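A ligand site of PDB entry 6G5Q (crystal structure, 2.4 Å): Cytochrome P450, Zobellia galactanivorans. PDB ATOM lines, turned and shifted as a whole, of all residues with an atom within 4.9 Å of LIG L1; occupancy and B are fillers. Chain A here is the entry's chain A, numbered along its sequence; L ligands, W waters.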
ATOM      1  N   PRO A  72     -25.318  14.844 -21.358  1.00  0.00           N
ATOM      2  CA  PRO A  72     -26.598  14.114 -21.277  1.00  0.00           C
ATOM      3  C   PRO A  72     -27.198  13.904 -19.857  1.00  0.00           C
ATOM      4  O   PRO A  72     -28.253  13.260 -19.708  1.00  0.00           O
ATOM      5  CB  PRO A  72     -26.237  12.714 -21.841  1.00  0.00           C
ATOM      6  CG  PRO A  72     -24.821  12.769 -22.253  1.00  0.00           C
ATOM      7  CD  PRO A  72     -24.204  13.895 -21.487  1.00  0.00           C
ATOM      8  N   PHE A  73     -26.543  14.439 -18.838  1.00  0.00           N
ATOM      9  CA  PHE A  73     -26.934  14.260 -17.443  1.00  0.00           C
ATOM     10  C   PHE A  73     -28.419  14.492 -17.092  1.00  0.00           C
ATOM     11  O   PHE A  73     -29.012  13.723 -16.314  1.00  0.00           O
ATOM     12  CB  PHE A  73     -26.037  15.164 -16.587  1.00  0.00           C
ATOM     13  CG  PHE A  73     -26.292  15.080 -15.098  1.00  0.00           C
ATOM     14  CD1 PHE A  73     -26.257  13.846 -14.419  1.00  0.00           C
ATOM     15  CD2 PHE A  73     -26.563  16.261 -14.381  1.00  0.00           C
ATOM     16  CE1 PHE A  73     -26.478  13.808 -13.044  1.00  0.00           C
ATOM     17  CE2 PHE A  73     -26.784  16.215 -13.012  1.00  0.00           C
ATOM     18  CZ  PHE A  73     -26.739  14.983 -12.353  1.00  0.00           C
ATOM     19  N   HIS A  80     -31.649  10.947 -24.539  1.00  0.00           N
ATOM     20  CA  HIS A  80     -30.364  10.710 -23.846  1.00  0.00           C
ATOM     21  C   HIS A  80     -29.322   9.947 -24.720  1.00  0.00           C
ATOM     22  O   HIS A  80     -28.171  10.395 -24.865  1.00  0.00           O
ATOM     23  CB  HIS A  80     -30.591  10.000 -22.507  1.00  0.00           C
ATOM     24  CG  HIS A  80     -29.320   9.582 -21.837  1.00  0.00           C
ATOM     25  ND1 HIS A  80     -28.716   8.351 -22.065  1.00  0.00           N
ATOM     26  CD2 HIS A  80     -28.496  10.253 -20.999  1.00  0.00           C
ATOM     27  CE1 HIS A  80     -27.591   8.292 -21.377  1.00  0.00           C
ATOM     28  NE2 HIS A  80     -27.443   9.411 -20.713  1.00  0.00           N
ATOM     29  N   ARG A  84     -25.607  11.151 -26.028  1.00  0.00           N
ATOM     30  CA  ARG A  84     -24.504  10.391 -25.522  1.00  0.00           C
ATOM     31  C   ARG A  84     -23.657   9.829 -26.666  1.00  0.00           C
ATOM     32  O   ARG A  84     -22.418   9.819 -26.556  1.00  0.00           O
ATOM     33  CB  ARG A  84     -25.010   9.245 -24.647  1.00  0.00           C
ATOM     34  CG  ARG A  84     -23.875   8.388 -24.114  1.00  0.00           C
ATOM     35  CD  ARG A  84     -24.131   7.943 -22.710  1.00  0.00           C
ATOM     36  NE  ARG A  84     -23.053   7.083 -22.235  1.00  0.00           N
ATOM     37  CZ  ARG A  84     -22.766   6.855 -20.966  1.00  0.00           C
ATOM     38  NH1 ARG A  84     -23.481   7.429 -20.002  1.00  0.00           N
ATOM     39  NH2 ARG A  84     -21.769   6.055 -20.649  1.00  0.00           N
ATOM     40  N   PHE A  91     -14.990  11.108 -25.147  1.00  0.00           N
ATOM     41  CA  PHE A  91     -14.678  10.605 -23.813  1.00  0.00           C
ATOM     42  C   PHE A  91     -13.851   9.310 -23.738  1.00  0.00           C
ATOM     43  O   PHE A  91     -13.341   8.993 -22.655  1.00  0.00           O
ATOM     44  CB  PHE A  91     -15.945  10.507 -22.939  1.00  0.00           C
ATOM     45  CG  PHE A  91     -16.390  11.813 -22.374  1.00  0.00           C
ATOM     46  CD1 PHE A  91     -15.818  12.328 -21.187  1.00  0.00           C
ATOM     47  CD2 PHE A  91     -17.388  12.556 -23.000  1.00  0.00           C
ATOM     48  CE1 PHE A  91     -16.236  13.564 -20.666  1.00  0.00           C
ATOM     49  CE2 PHE A  91     -17.819  13.791 -22.476  1.00  0.00           C
ATOM     50  CZ  PHE A  91     -17.253  14.291 -21.318  1.00  0.00           C
ATOM     51  N   LEU A 135      -7.105  17.564 -17.090  1.00  0.00           N
ATOM     52  CA  LEU A 135      -8.292  18.012 -17.791  1.00  0.00           C
ATOM     53  C   LEU A 135      -7.928  18.722 -19.074  1.00  0.00           C
ATOM     54  O   LEU A 135      -8.745  18.737 -19.995  1.00  0.00           O
ATOM     55  CB  LEU A 135      -9.202  18.912 -16.910  1.00  0.00           C
ATOM     56  CG  LEU A 135     -10.536  19.327 -17.570  1.00  0.00           C
ATOM     57  CD1 LEU A 135     -11.383  18.103 -17.934  1.00  0.00           C
ATOM     58  CD2 LEU A 135     -11.331  20.209 -16.676  1.00  0.00           C
ATOM     59  N   LEU A 138      -8.043  16.029 -21.783  1.00  0.00           N
ATOM     60  CA  LEU A 138      -9.400  15.689 -22.150  1.00  0.00           C
ATOM     61  C   LEU A 138     -10.103  16.746 -23.054  1.00  0.00           C
ATOM     62  O   LEU A 138     -10.775  16.403 -23.994  1.00  0.00           O
ATOM     63  CB  LEU A 138     -10.221  15.460 -20.904  1.00  0.00           C
ATOM     64  CG  LEU A 138     -11.627  14.881 -21.163  1.00  0.00           C
ATOM     65  CD1 LEU A 138     -11.522  13.539 -21.886  1.00  0.00           C
ATOM     66  CD2 LEU A 138     -12.407  14.740 -19.853  1.00  0.00           C
ATOM     67  N   LEU A 216     -21.328  20.492 -17.479  1.00  0.00           N
ATOM     68  CA  LEU A 216     -21.303  19.152 -16.925  1.00  0.00           C
ATOM     69  C   LEU A 216     -19.899  18.554 -16.896  1.00  0.00           C
ATOM     70  O   LEU A 216     -19.537  17.888 -15.950  1.00  0.00           O
ATOM     71  CB  LEU A 216     -22.281  18.268 -17.683  1.00  0.00           C
ATOM     72  CG  LEU A 216     -22.215  16.777 -17.432  1.00  0.00           C
ATOM     73  CD1 LEU A 216     -22.639  16.421 -16.015  1.00  0.00           C
ATOM     74  CD2 LEU A 216     -23.066  16.084 -18.491  1.00  0.00           C
ATOM     75  N   THR A 217     -19.107  18.820 -17.939  1.00  0.00           N
ATOM     76  CA  THR A 217     -17.769  18.255 -18.048  1.00  0.00           C
ATOM     77  C   THR A 217     -16.804  18.815 -16.972  1.00  0.00           C
ATOM     78  O   THR A 217     -16.066  18.029 -16.350  1.00  0.00           O
ATOM     79  CB  THR A 217     -17.219  18.410 -19.457  1.00  0.00           C
ATOM     80  OG1 THR A 217     -18.079  17.710 -20.371  1.00  0.00           O
ATOM     81  CG2 THR A 217     -15.795  17.845 -19.575  1.00  0.00           C
ATOM     82  N   GLY A 220     -18.598  17.822 -13.231  1.00  0.00           N
ATOM     83  CA  GLY A 220     -18.707  16.402 -12.942  1.00  0.00           C
ATOM     84  C   GLY A 220     -17.405  15.735 -12.511  1.00  0.00           C
ATOM     85  O   GLY A 220     -17.414  14.692 -11.800  1.00  0.00           O
ATOM     86  N   GLY A 221     -16.287  16.306 -12.919  1.00  0.00           N
ATOM     87  CA  GLY A 221     -15.028  15.648 -12.697  1.00  0.00           C
ATOM     88  C   GLY A 221     -14.089  16.339 -11.760  1.00  0.00           C
ATOM     89  O   GLY A 221     -12.981  15.860 -11.564  1.00  0.00           O
ATOM     90  N   THR A 224     -14.899  15.041  -7.493  1.00  0.00           N
ATOM     91  CA  THR A 224     -14.743  13.572  -7.530  1.00  0.00           C
ATOM     92  C   THR A 224     -13.272  13.156  -7.751  1.00  0.00           C
ATOM     93  O   THR A 224     -12.737  12.344  -7.010  1.00  0.00           O
ATOM     94  CB  THR A 224     -15.656  12.935  -8.608  1.00  0.00           C
ATOM     95  OG1 THR A 224     -15.410  13.574  -9.870  1.00  0.00           O
ATOM     96  CG2 THR A 224     -17.120  13.095  -8.263  1.00  0.00           C
ATOM     97  N   VAL A 225     -12.602  13.749  -8.752  1.00  0.00           N
ATOM     98  CA  VAL A 225     -11.227  13.355  -9.027  1.00  0.00           C
ATOM     99  C   VAL A 225     -10.298  13.773  -7.892  1.00  0.00           C
ATOM    100  O   VAL A 225      -9.399  13.006  -7.509  1.00  0.00           O
ATOM    101  CB  VAL A 225     -10.718  13.886 -10.401  1.00  0.00           C
ATOM    102  CG1 VAL A 225      -9.184  13.838 -10.517  1.00  0.00           C
ATOM    103  CG2 VAL A 225     -11.387  13.130 -11.558  1.00  0.00           C
ATOM    104  N   ALA A 228     -10.734  11.382  -5.071  1.00  0.00           N
ATOM    105  CA  ALA A 228     -10.150  10.089  -5.413  1.00  0.00           C
ATOM    106  C   ALA A 228      -8.619  10.140  -5.277  1.00  0.00           C
ATOM    107  O   ALA A 228      -8.009   9.271  -4.650  1.00  0.00           O
ATOM    108  CB  ALA A 228     -10.579   9.610  -6.811  1.00  0.00           C
ATOM    109  N   ILE A 261     -12.398   3.138  -6.105  1.00  0.00           N
ATOM    110  CA  ILE A 261     -13.608   3.859  -6.433  1.00  0.00           C
ATOM    111  C   ILE A 261     -14.809   3.275  -5.667  1.00  0.00           C
ATOM    112  O   ILE A 261     -15.644   4.027  -5.163  1.00  0.00           O
ATOM    113  CB  ILE A 261     -13.870   3.878  -7.943  1.00  0.00           C
ATOM    114  CG1 ILE A 261     -12.763   4.673  -8.700  1.00  0.00           C
ATOM    115  CG2 ILE A 261     -15.261   4.435  -8.219  1.00  0.00           C
ATOM    116  CD1 ILE A 261     -12.500   6.097  -8.236  1.00  0.00           C
ATOM    117  N   PRO A 266     -16.427   8.571  -4.489  1.00  0.00           N
ATOM    118  CA  PRO A 266     -16.302  10.030  -4.412  1.00  0.00           C
ATOM    119  C   PRO A 266     -17.563  10.812  -4.649  1.00  0.00           C
ATOM    120  O   PRO A 266     -17.657  11.936  -4.171  1.00  0.00           O
ATOM    121  CB  PRO A 266     -15.267  10.343  -5.488  1.00  0.00           C
ATOM    122  CG  PRO A 266     -14.413   9.110  -5.549  1.00  0.00           C
ATOM    123  CD  PRO A 266     -15.401   7.984  -5.379  1.00  0.00           C
ATOM    124  N   LEU A 267     -18.528  10.249  -5.387  1.00  0.00           N
ATOM    125  CA  LEU A 267     -19.845  10.883  -5.554  1.00  0.00           C
ATOM    126  C   LEU A 267     -20.840  10.081  -4.764  1.00  0.00           C
ATOM    127  O   LEU A 267     -21.216   8.962  -5.125  1.00  0.00           O
ATOM    128  CB  LEU A 267     -20.282  10.965  -7.034  1.00  0.00           C
ATOM    129  CG  LEU A 267     -21.596  11.639  -7.456  1.00  0.00           C
ATOM    130  CD1 LEU A 267     -21.790  12.950  -6.719  1.00  0.00           C
ATOM    131  CD2 LEU A 267     -21.522  11.869  -8.959  1.00  0.00           C
ATOM    132  N   MET A 270     -26.877  10.706  -6.026  1.00  0.00           N
ATOM    133  CA  MET A 270     -27.456  11.561  -7.023  1.00  0.00           C
ATOM    134  C   MET A 270     -28.956  11.360  -6.944  1.00  0.00           C
ATOM    135  O   MET A 270     -29.464  10.225  -6.787  1.00  0.00           O
ATOM    136  CB  MET A 270     -26.965  11.180  -8.411  1.00  0.00           C
ATOM    137  CG  MET A 270     -27.336  12.179  -9.484  1.00  0.00           C
ATOM    138  SD  MET A 270     -27.002  13.878  -8.960  1.00  0.00           S
ATOM    139  CE  MET A 270     -25.207  13.945  -9.034  1.00  0.00           C
ATOM    140  N   ARG A 272     -33.033  11.581  -8.234  1.00  0.00           N
ATOM    141  CA  ARG A 272     -33.981  11.422  -9.329  1.00  0.00           C
ATOM    142  C   ARG A 272     -35.322  12.060  -8.915  1.00  0.00           C
ATOM    143  O   ARG A 272     -35.612  12.200  -7.722  1.00  0.00           O
ATOM    144  CB  ARG A 272     -34.190   9.949  -9.648  1.00  0.00           C
ATOM    145  CG  ARG A 272     -32.969   9.211 -10.118  1.00  0.00           C
ATOM    146  CD  ARG A 272     -32.598   9.636 -11.539  1.00  0.00           C
ATOM    147  NE  ARG A 272     -31.609   8.748 -12.142  1.00  0.00           N
ATOM    148  CZ  ARG A 272     -30.279   8.940 -12.109  1.00  0.00           C
ATOM    149  NH1 ARG A 272     -29.756   9.979 -11.471  1.00  0.00           N
ATOM    150  NH2 ARG A 272     -29.474   8.054 -12.715  1.00  0.00           N
ATOM    151  N   TRP A 295     -24.905   5.790  -3.928  1.00  0.00           N
ATOM    152  CA  TRP A 295     -23.874   4.907  -4.439  1.00  0.00           C
ATOM    153  C   TRP A 295     -22.918   4.462  -3.322  1.00  0.00           C
ATOM    154  O   TRP A 295     -22.502   3.290  -3.260  1.00  0.00           O
ATOM    155  CB  TRP A 295     -23.050   5.586  -5.553  1.00  0.00           C
ATOM    156  CG  TRP A 295     -23.846   6.412  -6.558  1.00  0.00           C
ATOM    157  CD1 TRP A 295     -23.876   7.801  -6.642  1.00  0.00           C
ATOM    158  CD2 TRP A 295     -24.684   5.930  -7.615  1.00  0.00           C
ATOM    159  NE1 TRP A 295     -24.703   8.190  -7.678  1.00  0.00           N
ATOM    160  CE2 TRP A 295     -25.207   7.066  -8.305  1.00  0.00           C
ATOM    161  CE3 TRP A 295     -25.054   4.639  -8.064  1.00  0.00           C
ATOM    162  CZ2 TRP A 295     -26.083   6.968  -9.405  1.00  0.00           C
ATOM    163  CZ3 TRP A 295     -25.940   4.531  -9.150  1.00  0.00           C
ATOM    164  CH2 TRP A 295     -26.447   5.700  -9.819  1.00  0.00           C
ATOM    165  N   VAL A 321     -21.068   0.400  -7.895  1.00  0.00           N
ATOM    166  CA  VAL A 321     -21.796   1.437  -8.604  1.00  0.00           C
ATOM    167  C   VAL A 321     -21.195   2.848  -8.386  1.00  0.00           C
ATOM    168  O   VAL A 321     -21.890   3.835  -8.510  1.00  0.00           O
ATOM    169  CB  VAL A 321     -23.292   1.388  -8.244  1.00  0.00           C
ATOM    170  CG1 VAL A 321     -23.905   0.075  -8.742  1.00  0.00           C
ATOM    171  CG2 VAL A 321     -23.469   1.489  -6.740  1.00  0.00           C
ATOM    172  N   GLY A 322     -19.901   2.912  -8.045  1.00  0.00           N
ATOM    173  CA  GLY A 322     -19.153   4.166  -7.930  1.00  0.00           C
ATOM    174  C   GLY A 322     -19.219   5.123  -9.124  1.00  0.00           C
ATOM    175  O   GLY A 322     -19.136   6.331  -8.941  1.00  0.00           O
ATOM    176  N   PHE A 323     -19.339   4.581 -10.329  1.00  0.00           N
ATOM    177  CA  PHE A 323     -19.487   5.299 -11.579  1.00  0.00           C
ATOM    178  C   PHE A 323     -20.939   5.169 -12.068  1.00  0.00           C
ATOM    179  O   PHE A 323     -21.209   5.294 -13.283  1.00  0.00           O
ATOM    180  CB  PHE A 323     -18.539   4.745 -12.658  1.00  0.00           C
ATOM    181  CG  PHE A 323     -17.068   5.061 -12.437  1.00  0.00           C
ATOM    182  CD1 PHE A 323     -16.639   6.383 -12.251  1.00  0.00           C
ATOM    183  CD2 PHE A 323     -16.105   4.021 -12.413  1.00  0.00           C
ATOM    184  CE1 PHE A 323     -15.291   6.672 -12.066  1.00  0.00           C
ATOM    185  CE2 PHE A 323     -14.749   4.298 -12.230  1.00  0.00           C
ATOM    186  CZ  PHE A 323     -14.341   5.635 -12.063  1.00  0.00           C
ATOM    187  N   GLY A 324     -21.884   4.913 -11.143  1.00  0.00           N
ATOM    188  CA  GLY A 324     -23.297   4.806 -11.516  1.00  0.00           C
ATOM    189  C   GLY A 324     -23.639   3.464 -12.150  1.00  0.00           C
ATOM    190  O   GLY A 324     -22.894   2.487 -12.026  1.00  0.00           O
ATOM    191  N   HIS A 327     -28.079   3.666 -17.734  1.00  0.00           N
ATOM    192  CA  HIS A 327     -28.054   4.774 -18.685  1.00  0.00           C
ATOM    193  C   HIS A 327     -27.046   5.848 -18.452  1.00  0.00           C
ATOM    194  O   HIS A 327     -26.334   6.212 -19.385  1.00  0.00           O
ATOM    195  CB  HIS A 327     -29.468   5.373 -18.848  1.00  0.00           C
ATOM    196  CG  HIS A 327     -30.469   4.327 -19.254  1.00  0.00           C
ATOM    197  ND1 HIS A 327     -31.301   3.705 -18.334  1.00  0.00           N
ATOM    198  CD2 HIS A 327     -30.689   3.721 -20.449  1.00  0.00           C
ATOM    199  CE1 HIS A 327     -32.016   2.781 -18.960  1.00  0.00           C
ATOM    200  NE2 HIS A 327     -31.650   2.764 -20.240  1.00  0.00           N
ATOM    201  N   HIS A 328     -27.000   6.370 -17.229  1.00  0.00           N
ATOM    202  CA  HIS A 328     -26.160   7.528 -16.960  1.00  0.00           C
ATOM    203  C   HIS A 328     -24.744   7.181 -16.449  1.00  0.00           C
ATOM    204  O   HIS A 328     -24.071   8.047 -15.908  1.00  0.00           O
ATOM    205  CB  HIS A 328     -26.872   8.510 -16.006  1.00  0.00           C
ATOM    206  CG  HIS A 328     -28.086   9.148 -16.608  1.00  0.00           C
ATOM    207  ND1 HIS A 328     -28.009  10.276 -17.422  1.00  0.00           N
ATOM    208  CD2 HIS A 328     -29.404   8.811 -16.563  1.00  0.00           C
ATOM    209  CE1 HIS A 328     -29.219  10.587 -17.853  1.00  0.00           C
ATOM    210  NE2 HIS A 328     -30.082   9.729 -17.333  1.00  0.00           N
ATOM    211  N   ASN A 329     -24.311   5.922 -16.606  1.00  0.00           N
ATOM    212  CA  ASN A 329     -22.980   5.526 -16.105  1.00  0.00           C
ATOM    213  C   ASN A 329     -21.930   6.537 -16.595  1.00  0.00           C
ATOM    214  O   ASN A 329     -21.914   6.936 -17.766  1.00  0.00           O
ATOM    215  CB  ASN A 329     -22.588   4.082 -16.464  1.00  0.00           C
ATOM    216  CG  ASN A 329     -22.293   3.910 -17.932  1.00  0.00           C
ATOM    217  OD1 ASN A 329     -21.151   4.096 -18.395  1.00  0.00           O
ATOM    218  ND2 ASN A 329     -23.333   3.571 -18.695  1.00  0.00           N
ATOM    219  N   CYS A 330     -21.066   6.921 -15.659  1.00  0.00           N
ATOM    220  CA  CYS A 330     -20.104   8.007 -15.806  1.00  0.00           C
ATOM    221  C   CYS A 330     -19.336   8.058 -17.144  1.00  0.00           C
ATOM    222  O   CYS A 330     -18.545   7.165 -17.439  1.00  0.00           O
ATOM    223  CB  CYS A 330     -19.103   7.955 -14.650  1.00  0.00           C
ATOM    224  SG  CYS A 330     -17.861   9.269 -14.675  1.00  0.00           S
ATOM    225  N   LEU A 331     -19.521   9.133 -17.916  1.00  0.00           N
ATOM    226  CA  LEU A 331     -18.685   9.283 -19.108  1.00  0.00           C
ATOM    227  C   LEU A 331     -17.193   9.565 -18.810  1.00  0.00           C
ATOM    228  O   LEU A 331     -16.295   9.240 -19.623  1.00  0.00           O
ATOM    229  CB  LEU A 331     -19.238  10.356 -20.047  1.00  0.00           C
ATOM    230  CG  LEU A 331     -20.345   9.859 -21.012  1.00  0.00           C
ATOM    231  CD1 LEU A 331     -21.174  11.050 -21.515  1.00  0.00           C
ATOM    232  CD2 LEU A 331     -19.735   9.036 -22.170  1.00  0.00           C
ATOM    233  N   GLY A 332     -16.915  10.204 -17.664  1.00  0.00           N
ATOM    234  CA  GLY A 332     -15.553  10.556 -17.297  1.00  0.00           C
ATOM    235  C   GLY A 332     -14.758   9.353 -16.757  1.00  0.00           C
ATOM    236  O   GLY A 332     -13.584   9.528 -16.438  1.00  0.00           O
ATOM    237  N   HIS A 335     -11.258   8.585 -18.368  1.00  0.00           N
ATOM    238  CA  HIS A 335     -10.283   9.600 -17.902  1.00  0.00           C
ATOM    239  C   HIS A 335      -9.878   9.346 -16.425  1.00  0.00           C
ATOM    240  O   HIS A 335      -8.674   9.253 -16.101  1.00  0.00           O
ATOM    241  CB  HIS A 335     -10.876  10.988 -18.054  1.00  0.00           C
ATOM    242  CG  HIS A 335      -9.958  12.104 -17.686  1.00  0.00           C
ATOM    243  ND1 HIS A 335      -8.877  12.475 -18.475  1.00  0.00           N
ATOM    244  CD2 HIS A 335     -10.002  12.982 -16.649  1.00  0.00           C
ATOM    245  CE1 HIS A 335      -8.288  13.525 -17.923  1.00  0.00           C
ATOM    246  NE2 HIS A 335      -8.959  13.860 -16.825  1.00  0.00           N
ATOM    247  N   ALA A 336     -10.873   9.222 -15.556  1.00  0.00           N
ATOM    248  CA  ALA A 336     -10.605   8.985 -14.123  1.00  0.00           C
ATOM    249  C   ALA A 336      -9.752   7.723 -13.894  1.00  0.00           C
ATOM    250  O   ALA A 336      -8.751   7.746 -13.139  1.00  0.00           O
ATOM    251  CB  ALA A 336     -11.888   8.926 -13.333  1.00  0.00           C
HETATM  252  C1  LIG L   1     -21.935  10.633 -14.381  1.00  0.00           C
HETATM  253  C2  LIG L   1     -19.020   9.398 -10.682  1.00  0.00           C
HETATM  254  C3  LIG L   1     -15.328  11.621 -12.784  1.00  0.00           C
HETATM  255  C4  LIG L   1     -18.292  13.219 -16.179  1.00  0.00           C
HETATM  256  C5  LIG L   1     -21.450  10.104 -13.195  1.00  0.00           C
HETATM  257  C6  LIG L   1     -22.205   9.341 -12.260  1.00  0.00           C
HETATM  258  C7  LIG L   1     -21.367   9.016 -11.243  1.00  0.00           C
HETATM  259  C8  LIG L   1     -20.103   9.543 -11.520  1.00  0.00           C
HETATM  260  C9  LIG L   1     -21.706   8.205 -10.027  1.00  0.00           C
HETATM  261  C10 LIG L   1     -23.655   8.891 -12.305  1.00  0.00           C
HETATM  262  C11 LIG L   1     -24.573  10.119 -12.264  1.00  0.00           C
HETATM  263  C12 LIG L   1     -26.037   9.775 -12.315  1.00  0.00           C
HETATM  264  O1  LIG L   1     -26.855  10.718 -12.488  1.00  0.00           O
HETATM  265  O2  LIG L   1     -26.440   8.583 -12.208  1.00  0.00           O
HETATM  266  C13 LIG L   1     -17.762   9.896 -10.970  1.00  0.00           C
HETATM  267  C14 LIG L   1     -16.647   9.604 -10.155  1.00  0.00           C
HETATM  268  C15 LIG L   1     -15.578  10.223 -10.722  1.00  0.00           C
HETATM  269  C16 LIG L   1     -16.121  10.898 -11.933  1.00  0.00           C
HETATM  270  C17 LIG L   1     -16.690   8.808  -8.884  1.00  0.00           C
HETATM  271  C18 LIG L   1     -14.160  10.321 -10.238  1.00  0.00           C
HETATM  272  C19 LIG L   1     -13.477   9.338  -9.666  1.00  0.00           C
HETATM  273  C20 LIG L   1     -15.808  12.270 -13.897  1.00  0.00           C
HETATM  274  C21 LIG L   1     -15.017  13.070 -14.751  1.00  0.00           C
HETATM  275  C22 LIG L   1     -15.891  13.578 -15.709  1.00  0.00           C
HETATM  276  C23 LIG L   1     -17.185  13.018 -15.419  1.00  0.00           C
HETATM  277  C24 LIG L   1     -13.502  13.316 -14.589  1.00  0.00           C
HETATM  278  C25 LIG L   1     -15.595  14.427 -16.872  1.00  0.00           C
HETATM  279  C26 LIG L   1     -14.428  15.003 -17.072  1.00  0.00           C
HETATM  280  C27 LIG L   1     -19.527  12.579 -15.988  1.00  0.00           C
HETATM  281  C28 LIG L   1     -20.641  12.743 -16.949  1.00  0.00           C
HETATM  282  C29 LIG L   1     -21.655  12.001 -16.456  1.00  0.00           C
HETATM  283  C30 LIG L   1     -21.153  11.442 -15.180  1.00  0.00           C
HETATM  284  C31 LIG L   1     -20.646  13.550 -18.231  1.00  0.00           C
HETATM  285  C32 LIG L   1     -23.042  11.901 -17.090  1.00  0.00           C
HETATM  286  C33 LIG L   1     -23.182  10.687 -18.013  1.00  0.00           C
HETATM  287  C34 LIG L   1     -24.596  10.612 -18.564  1.00  0.00           C
HETATM  288  O3  LIG L   1     -25.509  11.263 -18.002  1.00  0.00           O
HETATM  289  O4  LIG L   1     -24.903   9.890 -19.562  1.00  0.00           O
HETATM  290  N1  LIG L   1     -20.170  10.224 -12.695  1.00  0.00           N
HETATM  291  N2  LIG L   1     -17.415  10.640 -12.029  1.00  0.00           N
HETATM  292  N3  LIG L   1     -17.094  12.276 -14.298  1.00  0.00           N
HETATM  293  N4  LIG L   1     -19.867  11.806 -14.973  1.00  0.00           N
HETATM  294 FE1  LIG L   1     -18.714  11.245 -13.566  1.00  0.00          FE
HETATM  295  C1  LG2 L   2     -23.594  18.171 -12.187  1.00  0.00           C
HETATM  296  C2  LG2 L   2     -23.177  16.841 -11.511  1.00  0.00           C
HETATM  297  C3  LG2 L   2     -22.812  15.772 -12.521  1.00  0.00           C
HETATM  298  C4  LG2 L   2     -23.740  19.243 -11.116  1.00  0.00           C
HETATM  299  C5  LG2 L   2     -22.794  13.483 -12.637  1.00  0.00           C
HETATM  300  O1  LG2 L   2     -22.451  14.586 -11.800  1.00  0.00           O
HETATM  301  O2  LG2 L   2     -21.979  16.984 -10.700  1.00  0.00           O
HETATM  302  C6  LG2 L   2     -22.366  17.856  -9.660  1.00  0.00           C
HETATM  303  O3  LG2 L   2     -21.423  17.820  -8.620  1.00  0.00           O
HETATM  304  C7  LG2 L   2     -22.429  19.232 -10.359  1.00  0.00           C
HETATM  305  O4  LG2 L   2     -22.316  20.322  -9.485  1.00  0.00           O
HETATM  306  O5  LG2 L   2     -23.943  20.561 -11.659  1.00  0.00           O
HETATM  307  O6  LG2 L   2     -22.570  18.563 -13.116  1.00  0.00           O
HETATM  308  O   HOH W   1     -25.930   6.052 -13.513  1.00  0.00           O
HETATM  309  O   HOH W   2     -28.852  11.505 -14.361  1.00  0.00           O
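FE1 of LIG L1 is bound by SG of Cys 330.
A ring nitrogen (ND1) of His 328 sits at hydrogen-bond distance from an oxygen (O3) of LIG L1 (2.7 Å).
NE2 of His 80 sits at hydrogen-bond distance from O4 of LIG L1, at 2.8 Å.
An oxygen (O4) of LIG L1 lies within salt-bridge range of the guanidinium group of Arg 84, 2.9 Å away.
NH2 of Arg 272 is in salt-bridge range of O2 of LIG L1.
An oxygen (O3) of LIG L1 lies close to the backbone NH (N) of Phe 73.
N of Gly 332 lies close to SG of Cys 330, at 3.3 Å.
The backbone NH (N) of Cys 330 is in hydrogen-bond range of the backbone carbonyl oxygen (O) of Phe 323 (2.9 Å).
ND1 of His 328 is in hydrogen-bond range of NE2 of His 80, 3.4 Å away.
O of His 327 lies within hydrogen-bond range of NH1 of Arg 84 (3.2 Å).
The backbone carbonyl oxygen (O) of Asn 329 lies within hydrogen-bond range of the guanidinium group (NH1) of Arg 84 (2.8 Å).
OG1 of Thr 224 is in hydrogen-bond range of O of Gly 220, 3.0 Å away.
The backbone carbonyl oxygen (O) of Gly 220 sits close to a nitrogen (N3) of LIG L1, at 3.5 Å.
Residues that only touch LIG L1: Trp 295 (3.3 Å), Gly 221 (3.3 Å), Gly 322 (3.4 Å), Met 270 (3.4 Å), Thr 224 (3.4 Å), Gly 332 (3.4 Å), Leu 138 (3.4 Å), Gly 324 (3.5 Å), Leu 216 (3.5 Å), Thr 217 (3.5 Å), Pro 72 (3.6 Å), Leu 267 (3.7 Å), Ile 261 (3.7 Å), Val 225 (3.7 Å), Phe 323 (3.7 Å), Pro 266 (3.8 Å), Leu 331 (3.9 Å), Phe 91 (3.9 Å), His 327 (3.95 Å) and Asn 329 (3.97 Å).
Hydrophobic or aromatic side chains that line LIG L1: Pro 72, Phe 73, His 80, Phe 91, Leu 138, Leu 216, Val 225, Ile 261, Pro 266, Leu 267, Met 270, Trp 295, Phe 323, His 328 and Leu 331.
Within 4 Å of LIG L1: Pro 72, Phe 73, His 80, Arg 84, Phe 91, Leu 138, Leu 216, Thr 217, Gly 220, Gly 221, Thr 224, Val 225, Ile 261, Pro 266, Leu 267, Met 270, Arg 272, Trp 295, Gly 322, Phe 323, Gly 324, His 327, His 328, Asn 329, Cys 330, Leu 331 and Gly 332.
Water W2 lies within hydrogen-bond range of O1 of LIG L1 (2.8 Å), O of Phe 73 (3.0 Å), NH1 of Arg 272 (3.4 Å) and ND1 of His 328 (3.4 Å).
Water W1 bridges an oxygen (O2) of LIG L1 and the backbone NH of Asn 329.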
